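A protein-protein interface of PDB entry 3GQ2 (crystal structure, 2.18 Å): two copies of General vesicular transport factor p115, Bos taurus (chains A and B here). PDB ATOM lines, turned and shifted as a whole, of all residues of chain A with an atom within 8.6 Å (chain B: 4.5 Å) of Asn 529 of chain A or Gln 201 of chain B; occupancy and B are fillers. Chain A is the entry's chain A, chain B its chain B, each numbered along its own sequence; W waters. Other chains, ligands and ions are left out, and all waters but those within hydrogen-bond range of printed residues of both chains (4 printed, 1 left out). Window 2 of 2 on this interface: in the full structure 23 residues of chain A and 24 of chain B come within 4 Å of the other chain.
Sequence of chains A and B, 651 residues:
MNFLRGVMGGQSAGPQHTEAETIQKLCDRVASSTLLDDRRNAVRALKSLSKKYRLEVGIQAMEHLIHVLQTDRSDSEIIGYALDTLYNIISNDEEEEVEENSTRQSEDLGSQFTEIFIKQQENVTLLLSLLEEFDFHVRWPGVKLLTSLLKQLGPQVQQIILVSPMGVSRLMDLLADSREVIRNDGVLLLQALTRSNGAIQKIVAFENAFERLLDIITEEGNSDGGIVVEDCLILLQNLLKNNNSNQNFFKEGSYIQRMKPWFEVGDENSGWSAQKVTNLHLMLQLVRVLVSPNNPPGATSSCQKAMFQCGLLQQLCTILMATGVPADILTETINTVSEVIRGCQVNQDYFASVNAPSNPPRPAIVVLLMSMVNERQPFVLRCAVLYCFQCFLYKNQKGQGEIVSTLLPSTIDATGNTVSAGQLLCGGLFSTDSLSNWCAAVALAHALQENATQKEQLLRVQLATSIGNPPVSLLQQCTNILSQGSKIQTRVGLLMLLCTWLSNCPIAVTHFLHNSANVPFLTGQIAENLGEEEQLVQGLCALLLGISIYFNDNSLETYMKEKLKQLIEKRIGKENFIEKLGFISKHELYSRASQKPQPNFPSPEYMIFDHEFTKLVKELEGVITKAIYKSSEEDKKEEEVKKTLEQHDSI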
ATOM      1  N   THR A 523      19.207 -11.850   7.309  1.00  0.00           N
ATOM      2  CA  THR A 523      18.296 -10.950   6.583  1.00  0.00           C
ATOM      3  C   THR A 523      18.149  -9.596   7.325  1.00  0.00           C
ATOM      4  O   THR A 523      18.158  -8.509   6.698  1.00  0.00           O
ATOM      5  CB  THR A 523      16.915 -11.589   6.370  1.00  0.00           C
ATOM      6  OG1 THR A 523      16.270 -11.736   7.621  1.00  0.00           O
ATOM      7  CG2 THR A 523      17.045 -12.955   5.734  1.00  0.00           C
ATOM      8  N   GLY A 524      18.066  -9.690   8.657  1.00  0.00           N
ATOM      9  CA  GLY A 524      18.106  -8.545   9.563  1.00  0.00           C
ATOM     10  C   GLY A 524      19.323  -7.647   9.425  1.00  0.00           C
ATOM     11  O   GLY A 524      19.204  -6.408   9.326  1.00  0.00           O
ATOM     12  N   GLN A 525      20.502  -8.251   9.422  1.00  0.00           N
ATOM     13  CA  GLN A 525      21.711  -7.475   9.264  1.00  0.00           C
ATOM     14  C   GLN A 525      21.759  -6.806   7.882  1.00  0.00           C
ATOM     15  O   GLN A 525      22.248  -5.689   7.748  1.00  0.00           O
ATOM     16  CB  GLN A 525      22.936  -8.354   9.461  1.00  0.00           C
ATOM     17  CG  GLN A 525      23.109  -8.839  10.861  1.00  0.00           C
ATOM     18  CD  GLN A 525      23.678  -7.779  11.767  1.00  0.00           C
ATOM     19  OE1 GLN A 525      24.880  -7.562  11.792  1.00  0.00           O
ATOM     20  NE2 GLN A 525      22.809  -7.114  12.527  1.00  0.00           N
ATOM     21  N   ILE A 526      21.265  -7.488   6.857  1.00  0.00           N
ATOM     22  CA  ILE A 526      21.417  -7.013   5.480  1.00  0.00           C
ATOM     23  C   ILE A 526      20.436  -5.862   5.232  1.00  0.00           C
ATOM     24  O   ILE A 526      20.761  -4.887   4.543  1.00  0.00           O
ATOM     25  CB  ILE A 526      21.214  -8.152   4.459  1.00  0.00           C
ATOM     26  CG1 ILE A 526      22.238  -9.261   4.704  1.00  0.00           C
ATOM     27  CG2 ILE A 526      21.399  -7.609   3.049  1.00  0.00           C
ATOM     28  CD1 ILE A 526      22.037 -10.511   3.923  1.00  0.00           C
ATOM     29  N   ALA A 527      19.262  -5.968   5.838  1.00  0.00           N
ATOM     30  CA  ALA A 527      18.199  -4.987   5.690  1.00  0.00           C
ATOM     31  C   ALA A 527      18.401  -3.713   6.548  1.00  0.00           C
ATOM     32  O   ALA A 527      17.840  -2.668   6.234  1.00  0.00           O
ATOM     33  CB  ALA A 527      16.816  -5.658   6.011  1.00  0.00           C
ATOM     34  N   GLU A 528      19.198  -3.789   7.611  1.00  0.00           N
ATOM     35  CA  GLU A 528      19.370  -2.673   8.534  1.00  0.00           C
ATOM     36  C   GLU A 528      20.136  -1.534   7.890  1.00  0.00           C
ATOM     37  O   GLU A 528      20.967  -1.762   7.006  1.00  0.00           O
ATOM     38  CB  GLU A 528      20.135  -3.168   9.761  1.00  0.00           C
ATOM     39  CG  GLU A 528      20.287  -2.223  10.934  1.00  0.00           C
ATOM     40  CD  GLU A 528      18.970  -1.672  11.486  1.00  0.00           C
ATOM     41  OE1 GLU A 528      18.625  -2.045  12.629  1.00  0.00           O
ATOM     42  OE2 GLU A 528      18.290  -0.870  10.789  1.00  0.00           O
ATOM     43  N   ASN A 529      19.879  -0.306   8.348  1.00  0.00           N
ATOM     44  CA  ASN A 529      20.556   0.854   7.832  1.00  0.00           C
ATOM     45  C   ASN A 529      21.891   0.981   8.561  1.00  0.00           C
ATOM     46  O   ASN A 529      22.104   1.942   9.299  1.00  0.00           O
ATOM     47  CB  ASN A 529      19.701   2.126   8.027  1.00  0.00           C
ATOM     48  CG  ASN A 529      20.158   3.287   7.139  1.00  0.00           C
ATOM     49  OD1 ASN A 529      21.003   3.093   6.275  1.00  0.00           O
ATOM     50  ND2 ASN A 529      19.587   4.496   7.334  1.00  0.00           N
ATOM     51  N   LEU A 530      22.801   0.023   8.361  1.00  0.00           N
ATOM     52  CA  LEU A 530      24.050   0.040   9.128  1.00  0.00           C
ATOM     53  C   LEU A 530      24.936   1.123   8.580  1.00  0.00           C
ATOM     54  O   LEU A 530      24.819   1.511   7.423  1.00  0.00           O
ATOM     55  CB  LEU A 530      24.754  -1.313   9.139  1.00  0.00           C
ATOM     56  CG  LEU A 530      24.082  -2.408   9.976  1.00  0.00           C
ATOM     57  CD1 LEU A 530      24.519  -3.789   9.521  1.00  0.00           C
ATOM     58  CD2 LEU A 530      24.395  -2.221  11.448  1.00  0.00           C
ATOM     59  N   GLY A 531      25.780   1.658   9.437  1.00  0.00           N
ATOM     60  CA  GLY A 531      26.693   2.722   9.062  1.00  0.00           C
ATOM     61  C   GLY A 531      27.913   2.181   8.363  1.00  0.00           C
ATOM     62  O   GLY A 531      28.161   0.958   8.341  1.00  0.00           O
ATOM     63  N   GLU A 532      28.703   3.100   7.830  1.00  0.00           N
ATOM     64  CA  GLU A 532      29.814   2.747   6.974  1.00  0.00           C
ATOM     65  C   GLU A 532      30.832   1.807   7.634  1.00  0.00           C
ATOM     66  O   GLU A 532      31.372   0.923   6.983  1.00  0.00           O
ATOM     67  CB  GLU A 532      30.488   4.008   6.420  1.00  0.00           C
ATOM     68  CG  GLU A 532      31.652   3.662   5.453  1.00  0.00           C
ATOM     69  CD  GLU A 532      31.771   4.589   4.235  1.00  0.00           C
ATOM     70  OE1 GLU A 532      30.865   5.433   4.002  1.00  0.00           O
ATOM     71  OE2 GLU A 532      32.786   4.450   3.508  1.00  0.00           O
ATOM     72  N   GLU A 533      31.069   1.962   8.929  1.00  0.00           N
ATOM     73  CA  GLU A 533      32.076   1.128   9.589  1.00  0.00           C
ATOM     74  C   GLU A 533      31.685  -0.336   9.650  1.00  0.00           C
ATOM     75  O   GLU A 533      32.507  -1.144  10.027  1.00  0.00           O
ATOM     76  CB  GLU A 533      32.415   1.636  10.998  1.00  0.00           C
ATOM     77  CG  GLU A 533      31.394   1.267  12.075  1.00  0.00           C
ATOM     78  CD  GLU A 533      30.158   2.152  12.066  1.00  0.00           C
ATOM     79  OE1 GLU A 533      30.311   3.389  12.058  1.00  0.00           O
ATOM     80  OE2 GLU A 533      29.035   1.621  12.093  1.00  0.00           O
ATOM     81  N   GLU A 534      30.453  -0.663   9.261  1.00  0.00           N
ATOM     82  CA  GLU A 534      29.888  -2.014   9.379  1.00  0.00           C
ATOM     83  C   GLU A 534      29.370  -2.588   8.070  1.00  0.00           C
ATOM     84  O   GLU A 534      28.744  -3.659   8.061  1.00  0.00           O
ATOM     85  CB  GLU A 534      28.683  -1.957  10.302  1.00  0.00           C
ATOM     86  CG  GLU A 534      28.541  -3.120  11.247  1.00  0.00           C
ATOM     87  CD  GLU A 534      28.599  -2.661  12.671  1.00  0.00           C
ATOM     88  OE1 GLU A 534      29.489  -3.135  13.417  1.00  0.00           O
ATOM     89  OE2 GLU A 534      27.751  -1.805  13.023  1.00  0.00           O
ATOM     90  N   GLN A 535      29.620  -1.901   6.965  1.00  0.00           N
ATOM     91  CA  GLN A 535      29.114  -2.362   5.677  1.00  0.00           C
ATOM     92  C   GLN A 535      29.844  -3.543   5.056  1.00  0.00           C
ATOM     93  O   GLN A 535      29.227  -4.320   4.353  1.00  0.00           O
ATOM     94  CB  GLN A 535      28.993  -1.212   4.696  1.00  0.00           C
ATOM     95  CG  GLN A 535      27.719  -0.459   4.914  1.00  0.00           C
ATOM     96  CD  GLN A 535      27.663   0.823   4.130  1.00  0.00           C
ATOM     97  OE1 GLN A 535      28.679   1.505   3.951  1.00  0.00           O
ATOM     98  NE2 GLN A 535      26.458   1.175   3.671  1.00  0.00           N
ATOM     99  N   GLN A 538      28.106  -6.515   6.592  1.00  0.00           N
ATOM    100  CA  GLN A 538      26.791  -6.563   5.950  1.00  0.00           C
ATOM    101  C   GLN A 538      26.890  -7.254   4.604  1.00  0.00           C
ATOM    102  O   GLN A 538      26.096  -8.128   4.269  1.00  0.00           O
ATOM    103  CB  GLN A 538      26.261  -5.136   5.788  1.00  0.00           C
ATOM    104  CG  GLN A 538      24.788  -5.038   5.545  1.00  0.00           C
ATOM    105  CD  GLN A 538      24.271  -3.592   5.620  1.00  0.00           C
ATOM    106  OE1 GLN A 538      24.993  -2.634   5.331  1.00  0.00           O
ATOM    107  NE2 GLN A 538      23.008  -3.444   6.001  1.00  0.00           N
ATOM    108  N   ASN A 576      18.892  -4.541  -3.899  1.00  0.00           N
ATOM    109  CA  ASN A 576      19.483  -4.137  -2.633  1.00  0.00           C
ATOM    110  C   ASN A 576      20.473  -5.171  -2.116  1.00  0.00           C
ATOM    111  O   ASN A 576      21.621  -4.856  -1.790  1.00  0.00           O
ATOM    112  CB  ASN A 576      18.374  -3.955  -1.614  1.00  0.00           C
ATOM    113  CG  ASN A 576      18.566  -2.739  -0.787  1.00  0.00           C
ATOM    114  OD1 ASN A 576      19.403  -2.720   0.127  1.00  0.00           O
ATOM    115  ND2 ASN A 576      17.802  -1.685  -1.107  1.00  0.00           N
ATOM    116  N   LYS A 580      24.568  -4.800  -1.434  1.00  0.00           N
ATOM    117  CA  LYS A 580      25.252  -5.277  -0.210  1.00  0.00           C
ATOM    118  C   LYS A 580      26.309  -6.305  -0.576  1.00  0.00           C
ATOM    119  O   LYS A 580      27.432  -6.234  -0.094  1.00  0.00           O
ATOM    120  CB  LYS A 580      24.306  -5.925   0.833  1.00  0.00           C
ATOM    121  CG  LYS A 580      23.241  -5.007   1.505  1.00  0.00           C
ATOM    122  CD  LYS A 580      23.577  -3.534   1.438  1.00  0.00           C
ATOM    123  CE  LYS A 580      22.781  -2.661   2.429  1.00  0.00           C
ATOM    124  NZ  LYS A 580      21.541  -2.090   1.881  1.00  0.00           N
ATOM    125  N   THR B 194      18.791   6.788  17.360  1.00  0.00           N
ATOM    126  CA  THR B 194      18.569   6.684  15.911  1.00  0.00           C
ATOM    127  C   THR B 194      19.738   6.020  15.157  1.00  0.00           C
ATOM    128  O   THR B 194      19.556   5.534  14.042  1.00  0.00           O
ATOM    129  CB  THR B 194      18.323   8.063  15.291  1.00  0.00           C
ATOM    130  OG1 THR B 194      19.426   8.918  15.606  1.00  0.00           O
ATOM    131  CG2 THR B 194      17.030   8.674  15.842  1.00  0.00           C
ATOM    132  N   SER B 196      22.271   4.015  13.244  1.00  0.00           N
ATOM    133  CA  SER B 196      22.392   2.717  12.578  1.00  0.00           C
ATOM    134  C   SER B 196      21.118   1.878  12.696  1.00  0.00           C
ATOM    135  O   SER B 196      21.143   0.654  12.511  1.00  0.00           O
ATOM    136  CB  SER B 196      23.634   1.962  13.089  1.00  0.00           C
ATOM    137  OG  SER B 196      24.811   2.665  12.722  1.00  0.00           O
ATOM    138  N   ASN B 197      19.985   2.545  12.950  1.00  0.00           N
ATOM    139  CA  ASN B 197      18.739   1.834  13.207  1.00  0.00           C
ATOM    140  C   ASN B 197      17.594   2.388  12.414  1.00  0.00           C
ATOM    141  O   ASN B 197      16.926   3.337  12.854  1.00  0.00           O
ATOM    142  CB  ASN B 197      18.408   1.904  14.683  1.00  0.00           C
ATOM    143  CG  ASN B 197      17.279   0.975  15.059  1.00  0.00           C
ATOM    144  OD1 ASN B 197      16.285   0.859  14.348  1.00  0.00           O
ATOM    145  ND2 ASN B 197      17.436   0.303  16.175  1.00  0.00           N
ATOM    146  N   GLY B 198      17.342   1.781  11.260  1.00  0.00           N
ATOM    147  CA  GLY B 198      16.304   2.243  10.343  1.00  0.00           C
ATOM    148  C   GLY B 198      14.859   2.240  10.843  1.00  0.00           C
ATOM    149  O   GLY B 198      14.125   3.167  10.554  1.00  0.00           O
ATOM    150  N   ALA B 199      14.433   1.191  11.541  1.00  0.00           N
ATOM    151  CA  ALA B 199      13.090   1.168  12.128  1.00  0.00           C
ATOM    152  C   ALA B 199      12.860   2.407  13.001  1.00  0.00           C
ATOM    153  O   ALA B 199      11.879   3.115  12.805  1.00  0.00           O
ATOM    154  CB  ALA B 199      12.883  -0.098  12.957  1.00  0.00           C
ATOM    155  N   ILE B 200      13.786   2.677  13.935  1.00  0.00           N
ATOM    156  CA  ILE B 200      13.700   3.852  14.819  1.00  0.00           C
ATOM    157  C   ILE B 200      13.745   5.176  14.022  1.00  0.00           C
ATOM    158  O   ILE B 200      13.039   6.137  14.379  1.00  0.00           O
ATOM    159  CB  ILE B 200      14.802   3.840  15.957  1.00  0.00           C
ATOM    160  CG1 ILE B 200      14.750   2.567  16.851  1.00  0.00           C
ATOM    161  CG2 ILE B 200      14.697   5.057  16.862  1.00  0.00           C
ATOM    162  CD1 ILE B 200      13.398   1.941  16.997  1.00  0.00           C
ATOM    163  N   GLN B 201      14.541   5.240  12.944  1.00  0.00           N
ATOM    164  CA  GLN B 201      14.650   6.479  12.161  1.00  0.00           C
ATOM    165  C   GLN B 201      13.291   6.844  11.572  1.00  0.00           C
ATOM    166  O   GLN B 201      12.926   8.011  11.533  1.00  0.00           O
ATOM    167  CB  GLN B 201      15.718   6.388  11.044  1.00  0.00           C
ATOM    168  CG  GLN B 201      17.160   6.386  11.554  1.00  0.00           C
ATOM    169  CD  GLN B 201      18.178   5.664  10.644  1.00  0.00           C
ATOM    170  OE1 GLN B 201      17.844   5.168   9.553  1.00  0.00           O
ATOM    171  NE2 GLN B 201      19.439   5.614  11.106  1.00  0.00           N
ATOM    172  N   LYS B 202      12.568   5.834  11.093  1.00  0.00           N
ATOM    173  CA  LYS B 202      11.214   5.998  10.559  1.00  0.00           C
ATOM    174  C   LYS B 202      10.231   6.502  11.644  1.00  0.00           C
ATOM    175  O   LYS B 202       9.534   7.505  11.450  1.00  0.00           O
ATOM    176  CB  LYS B 202      10.732   4.655   9.965  1.00  0.00           C
ATOM    177  CG  LYS B 202       9.326   4.664   9.366  1.00  0.00           C
ATOM    178  CD  LYS B 202       8.899   3.294   8.765  1.00  0.00           C
ATOM    179  CE  LYS B 202       9.304   3.109   7.297  1.00  0.00           C
ATOM    180  NZ  LYS B 202       9.119   4.367   6.494  1.00  0.00           N
ATOM    181  N   ILE B 203      10.179   5.819  12.787  1.00  0.00           N
ATOM    182  CA  ILE B 203       9.293   6.254  13.889  1.00  0.00           C
ATOM    183  C   ILE B 203       9.614   7.702  14.321  1.00  0.00           C
ATOM    184  O   ILE B 203       8.718   8.477  14.558  1.00  0.00           O
ATOM    185  CB  ILE B 203       9.376   5.354  15.140  1.00  0.00           C
ATOM    186  CG1 ILE B 203       9.110   3.891  14.813  1.00  0.00           C
ATOM    187  CG2 ILE B 203       8.345   5.782  16.163  1.00  0.00           C
ATOM    188  CD1 ILE B 203       9.378   2.960  16.031  1.00  0.00           C
ATOM    189  N   VAL B 204      10.895   8.050  14.392  1.00  0.00           N
ATOM    190  CA  VAL B 204      11.297   9.383  14.780  1.00  0.00           C
ATOM    191  C   VAL B 204      10.817  10.444  13.770  1.00  0.00           C
ATOM    192  O   VAL B 204      10.383  11.532  14.183  1.00  0.00           O
ATOM    193  CB  VAL B 204      12.818   9.459  15.031  1.00  0.00           C
ATOM    194  CG1 VAL B 204      13.300  10.903  14.987  1.00  0.00           C
ATOM    195  CG2 VAL B 204      13.144   8.816  16.389  1.00  0.00           C
ATOM    196  N   ALA B 205      10.861  10.102  12.475  1.00  0.00           N
ATOM    197  CA  ALA B 205      10.340  10.960  11.398  1.00  0.00           C
ATOM    198  C   ALA B 205       8.830  11.048  11.457  1.00  0.00           C
ATOM    199  O   ALA B 205       8.263  12.114  11.234  1.00  0.00           O
ATOM    200  CB  ALA B 205      10.758  10.460  10.039  1.00  0.00           C
ATOM    201  N   ASN B 238      21.345  11.336  10.538  1.00  0.00           N
ATOM    202  CA  ASN B 238      20.960   9.990  10.995  1.00  0.00           C
ATOM    203  C   ASN B 238      19.627   9.581  10.397  1.00  0.00           C
ATOM    204  O   ASN B 238      19.423   8.427  10.100  1.00  0.00           O
ATOM    205  CB  ASN B 238      20.840   9.880  12.518  1.00  0.00           C
ATOM    206  CG  ASN B 238      22.162   9.930  13.227  1.00  0.00           C
ATOM    207  OD1 ASN B 238      23.197  10.261  12.647  1.00  0.00           O
ATOM    208  ND2 ASN B 238      22.137   9.607  14.506  1.00  0.00           N
ATOM    209  N   LEU B 239      18.720  10.535  10.235  1.00  0.00           N
ATOM    210  CA  LEU B 239      17.370  10.230   9.792  1.00  0.00           C
ATOM    211  C   LEU B 239      17.277  10.023   8.290  1.00  0.00           C
ATOM    212  O   LEU B 239      16.435   9.235   7.838  1.00  0.00           O
ATOM    213  CB  LEU B 239      16.389  11.341  10.235  1.00  0.00           C
ATOM    214  CG  LEU B 239      16.065  11.403  11.740  1.00  0.00           C
ATOM    215  CD1 LEU B 239      15.101  12.587  12.070  1.00  0.00           C
ATOM    216  CD2 LEU B 239      15.497  10.062  12.264  1.00  0.00           C
ATOM    217  N   LYS B 241      20.298   9.679   5.952  1.00  0.00           N
ATOM    218  CA  LYS B 241      21.411   9.027   5.256  1.00  0.00           C
ATOM    219  C   LYS B 241      21.089   7.578   5.008  1.00  0.00           C
ATOM    220  O   LYS B 241      20.832   6.844   5.957  1.00  0.00           O
ATOM    221  CB  LYS B 241      22.743   9.145   6.000  1.00  0.00           C
ATOM    222  CG  LYS B 241      23.939   8.656   5.159  1.00  0.00           C
ATOM    223  CD  LYS B 241      25.287   9.045   5.706  1.00  0.00           C
ATOM    224  CE  LYS B 241      26.406   8.554   4.805  1.00  0.00           C
ATOM    225  NZ  LYS B 241      27.748   8.942   5.351  1.00  0.00           N
ATOM    226  N   ASN B 242      21.059   7.212   3.714  1.00  0.00           N
ATOM    227  CA  ASN B 242      20.752   5.854   3.213  1.00  0.00           C
ATOM    228  C   ASN B 242      19.403   5.306   3.669  1.00  0.00           C
ATOM    229  O   ASN B 242      19.205   4.094   3.691  1.00  0.00           O
ATOM    230  CB  ASN B 242      21.827   4.821   3.614  1.00  0.00           C
ATOM    231  CG  ASN B 242      23.224   5.204   3.189  1.00  0.00           C
ATOM    232  OD1 ASN B 242      23.424   5.954   2.235  1.00  0.00           O
ATOM    233  ND2 ASN B 242      24.220   4.662   3.908  1.00  0.00           N
ATOM    234  N   ASN B 243      18.485   6.182   4.038  1.00  0.00           N
ATOM    235  CA  ASN B 243      17.159   5.788   4.499  1.00  0.00           C
ATOM    236  C   ASN B 243      16.184   6.282   3.453  1.00  0.00           C
ATOM    237  O   ASN B 243      15.835   7.473   3.463  1.00  0.00           O
ATOM    238  CB  ASN B 243      16.889   6.406   5.880  1.00  0.00           C
ATOM    239  CG  ASN B 243      15.590   5.907   6.526  1.00  0.00           C
ATOM    240  OD1 ASN B 243      14.548   5.885   5.886  1.00  0.00           O
ATOM    241  ND2 ASN B 243      15.662   5.492   7.803  1.00  0.00           N
ATOM    242  N   ASN B 246      12.404   7.859   4.556  1.00  0.00           N
ATOM    243  CA  ASN B 246      12.563   9.179   5.142  1.00  0.00           C
ATOM    244  C   ASN B 246      12.984  10.276   4.145  1.00  0.00           C
ATOM    245  O   ASN B 246      12.446  11.406   4.175  1.00  0.00           O
ATOM    246  CB  ASN B 246      13.559   9.108   6.302  1.00  0.00           C
ATOM    247  CG  ASN B 246      12.925   8.611   7.625  1.00  0.00           C
ATOM    248  OD1 ASN B 246      11.744   8.310   7.690  1.00  0.00           O
ATOM    249  ND2 ASN B 246      13.723   8.584   8.686  1.00  0.00           N
HETATM  250  O   HOH W   1      21.919   4.538   9.661  1.00  0.00           O
HETATM  251  O   HOH W   2      26.649   0.973  12.338  1.00  0.00           O
HETATM  252  O   HOH W   3      23.707   3.615   6.539  1.00  0.00           O
HETATM  253  O   HOH W   4      15.810  -1.360  11.552  1.00  0.00           O
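OE2 of Glu 528 of chain A is in hydrogen-bond range of N of Gly 198 of chain B. The side-chain amide nitrogen (ND2) of Asn 529 of chain A is in hydrogen-bond range of the side-chain amide oxygen (OE1) of Gln 201 of chain B. The side-chain amide nitrogen (ND2) of Asn 529 of chain A is in hydrogen-bond range of the backbone carbonyl oxygen (O) of Lys 241 of chain B, 3.0 Å away. O of Asn 242 of chain B lies close to OD1 of Asn 529 of chain A.
The side-chain amide nitrogen of Gln 538 of chain A is in hydrogen-bond range of the backbone carbonyl oxygen of Glu 528 of chain A, at 2.8 Å. The backbone carbonyl oxygen (O) of Thr 194 of chain B sits at hydrogen-bond distance from the side-chain amide nitrogen (NE2) of Gln 201 of chain B. N of Ala 199 of chain B sits at hydrogen-bond distance from OD1 of Asn 197 of chain B, 3.4 Å away. O of Asn 238 of chain B lies within hydrogen-bond range of NE2 of Gln 201 of chain B (3.0 Å). O of Gln 201 of chain B sits at hydrogen-bond distance from ND2 of Asn 246 of chain B, 3.0 Å away. OD1 of Asn 243 of chain B is in hydrogen-bond range of N of Asn 246 of chain B (3.2 Å).
Ser 196 of chain B touches Glu 528 of chain A (O to CD, 3.3 Å). CA of Asn 197 of chain B touches OE2 of Glu 528 of chain A, at 3.7 Å. Asn 529 of chain A touches Ser 196 of chain B. ND2 of Asn 529 of chain A touches CB of Asn 243 of chain B, at 3.6 Å. OG of Ser 196 of chain B touches N of Gly 531 of chain A, at 3.6 Å.
Of the printed residues of chain B, Asn 529 of chain A touches Ser 196 (3.4 Å), Gln 201 (2.9 Å), Lys 241 (3.0 Å), Asn 242 (3.3 Å) and Asn 243 (3.6 Å). Of the printed residues of chain A, Gln 201 of chain B touches Asn 529. Of chain A, only Glu 528 (3.3 Å), Asn 529 (3.4 Å) and Gly 531 (3.6 Å) come within 4 Å of Ser 196 of chain B. Printed residues of chain A within 4 Å of Asn 243 of chain B: Asn 529. Of the printed residues of chain A, Asn 242 of chain B touches Asn 529. Printed residues of chain B within 4 Å of Glu 528 of chain A: Ser 196 (3.3 Å), Asn 197 (3.7 Å) and Gly 198 (2.9 Å). Of the printed residues of chain B, Gly 531 of chain A touches Ser 196. Printed residues of chain A within 4 Å of Asn 197 of chain B: Glu 528. The nearest printed residue of chain B that does not touch Asn 529 of chain A is Gly 198 of chain B (4.02 Å). The nearest residue of chain A that does not touch Gln 201 of chain B is Glu 528 of chain A (6.2 Å). The nearest printed residue of chain B that does not touch Glu 528 of chain A is Ala 199 of chain B (4.4 Å).
Along chain A the printed residues that touch a printed residue of chain B span positions 528 to 531. Among the printed residues, 9 pairs touch across the chains.
No position is printed for both chains.
Water W2 lies within hydrogen-bond range of OE2 of Glu 533 of chain A, OG of Ser 196 of chain B, OE2 of Glu 534 of chain A and N of Gly 531 of chain A. Water W3 lies within hydrogen-bond range of the backbone carbonyl oxygen (O) of Leu 530 of chain A (2.5 Å), the side-chain amide oxygen (OD1) of Asn 529 of chain A (2.8 Å) and the side-chain amide nitrogen (ND2) of Asn 242 of chain B (2.9 Å). Water W1 lies within hydrogen-bond range of the backbone carbonyl oxygen (O) of Asn 529 of chain A (2.6 Å) and the side-chain amide nitrogen (NE2) of Gln 201 of chain B (3.1 Å). Water W4 bridges the side-chain carboxylate of Glu 528 of chain A (2.6 Å) and the backbone NH of Ala 199 of chain B (2.9 Å).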
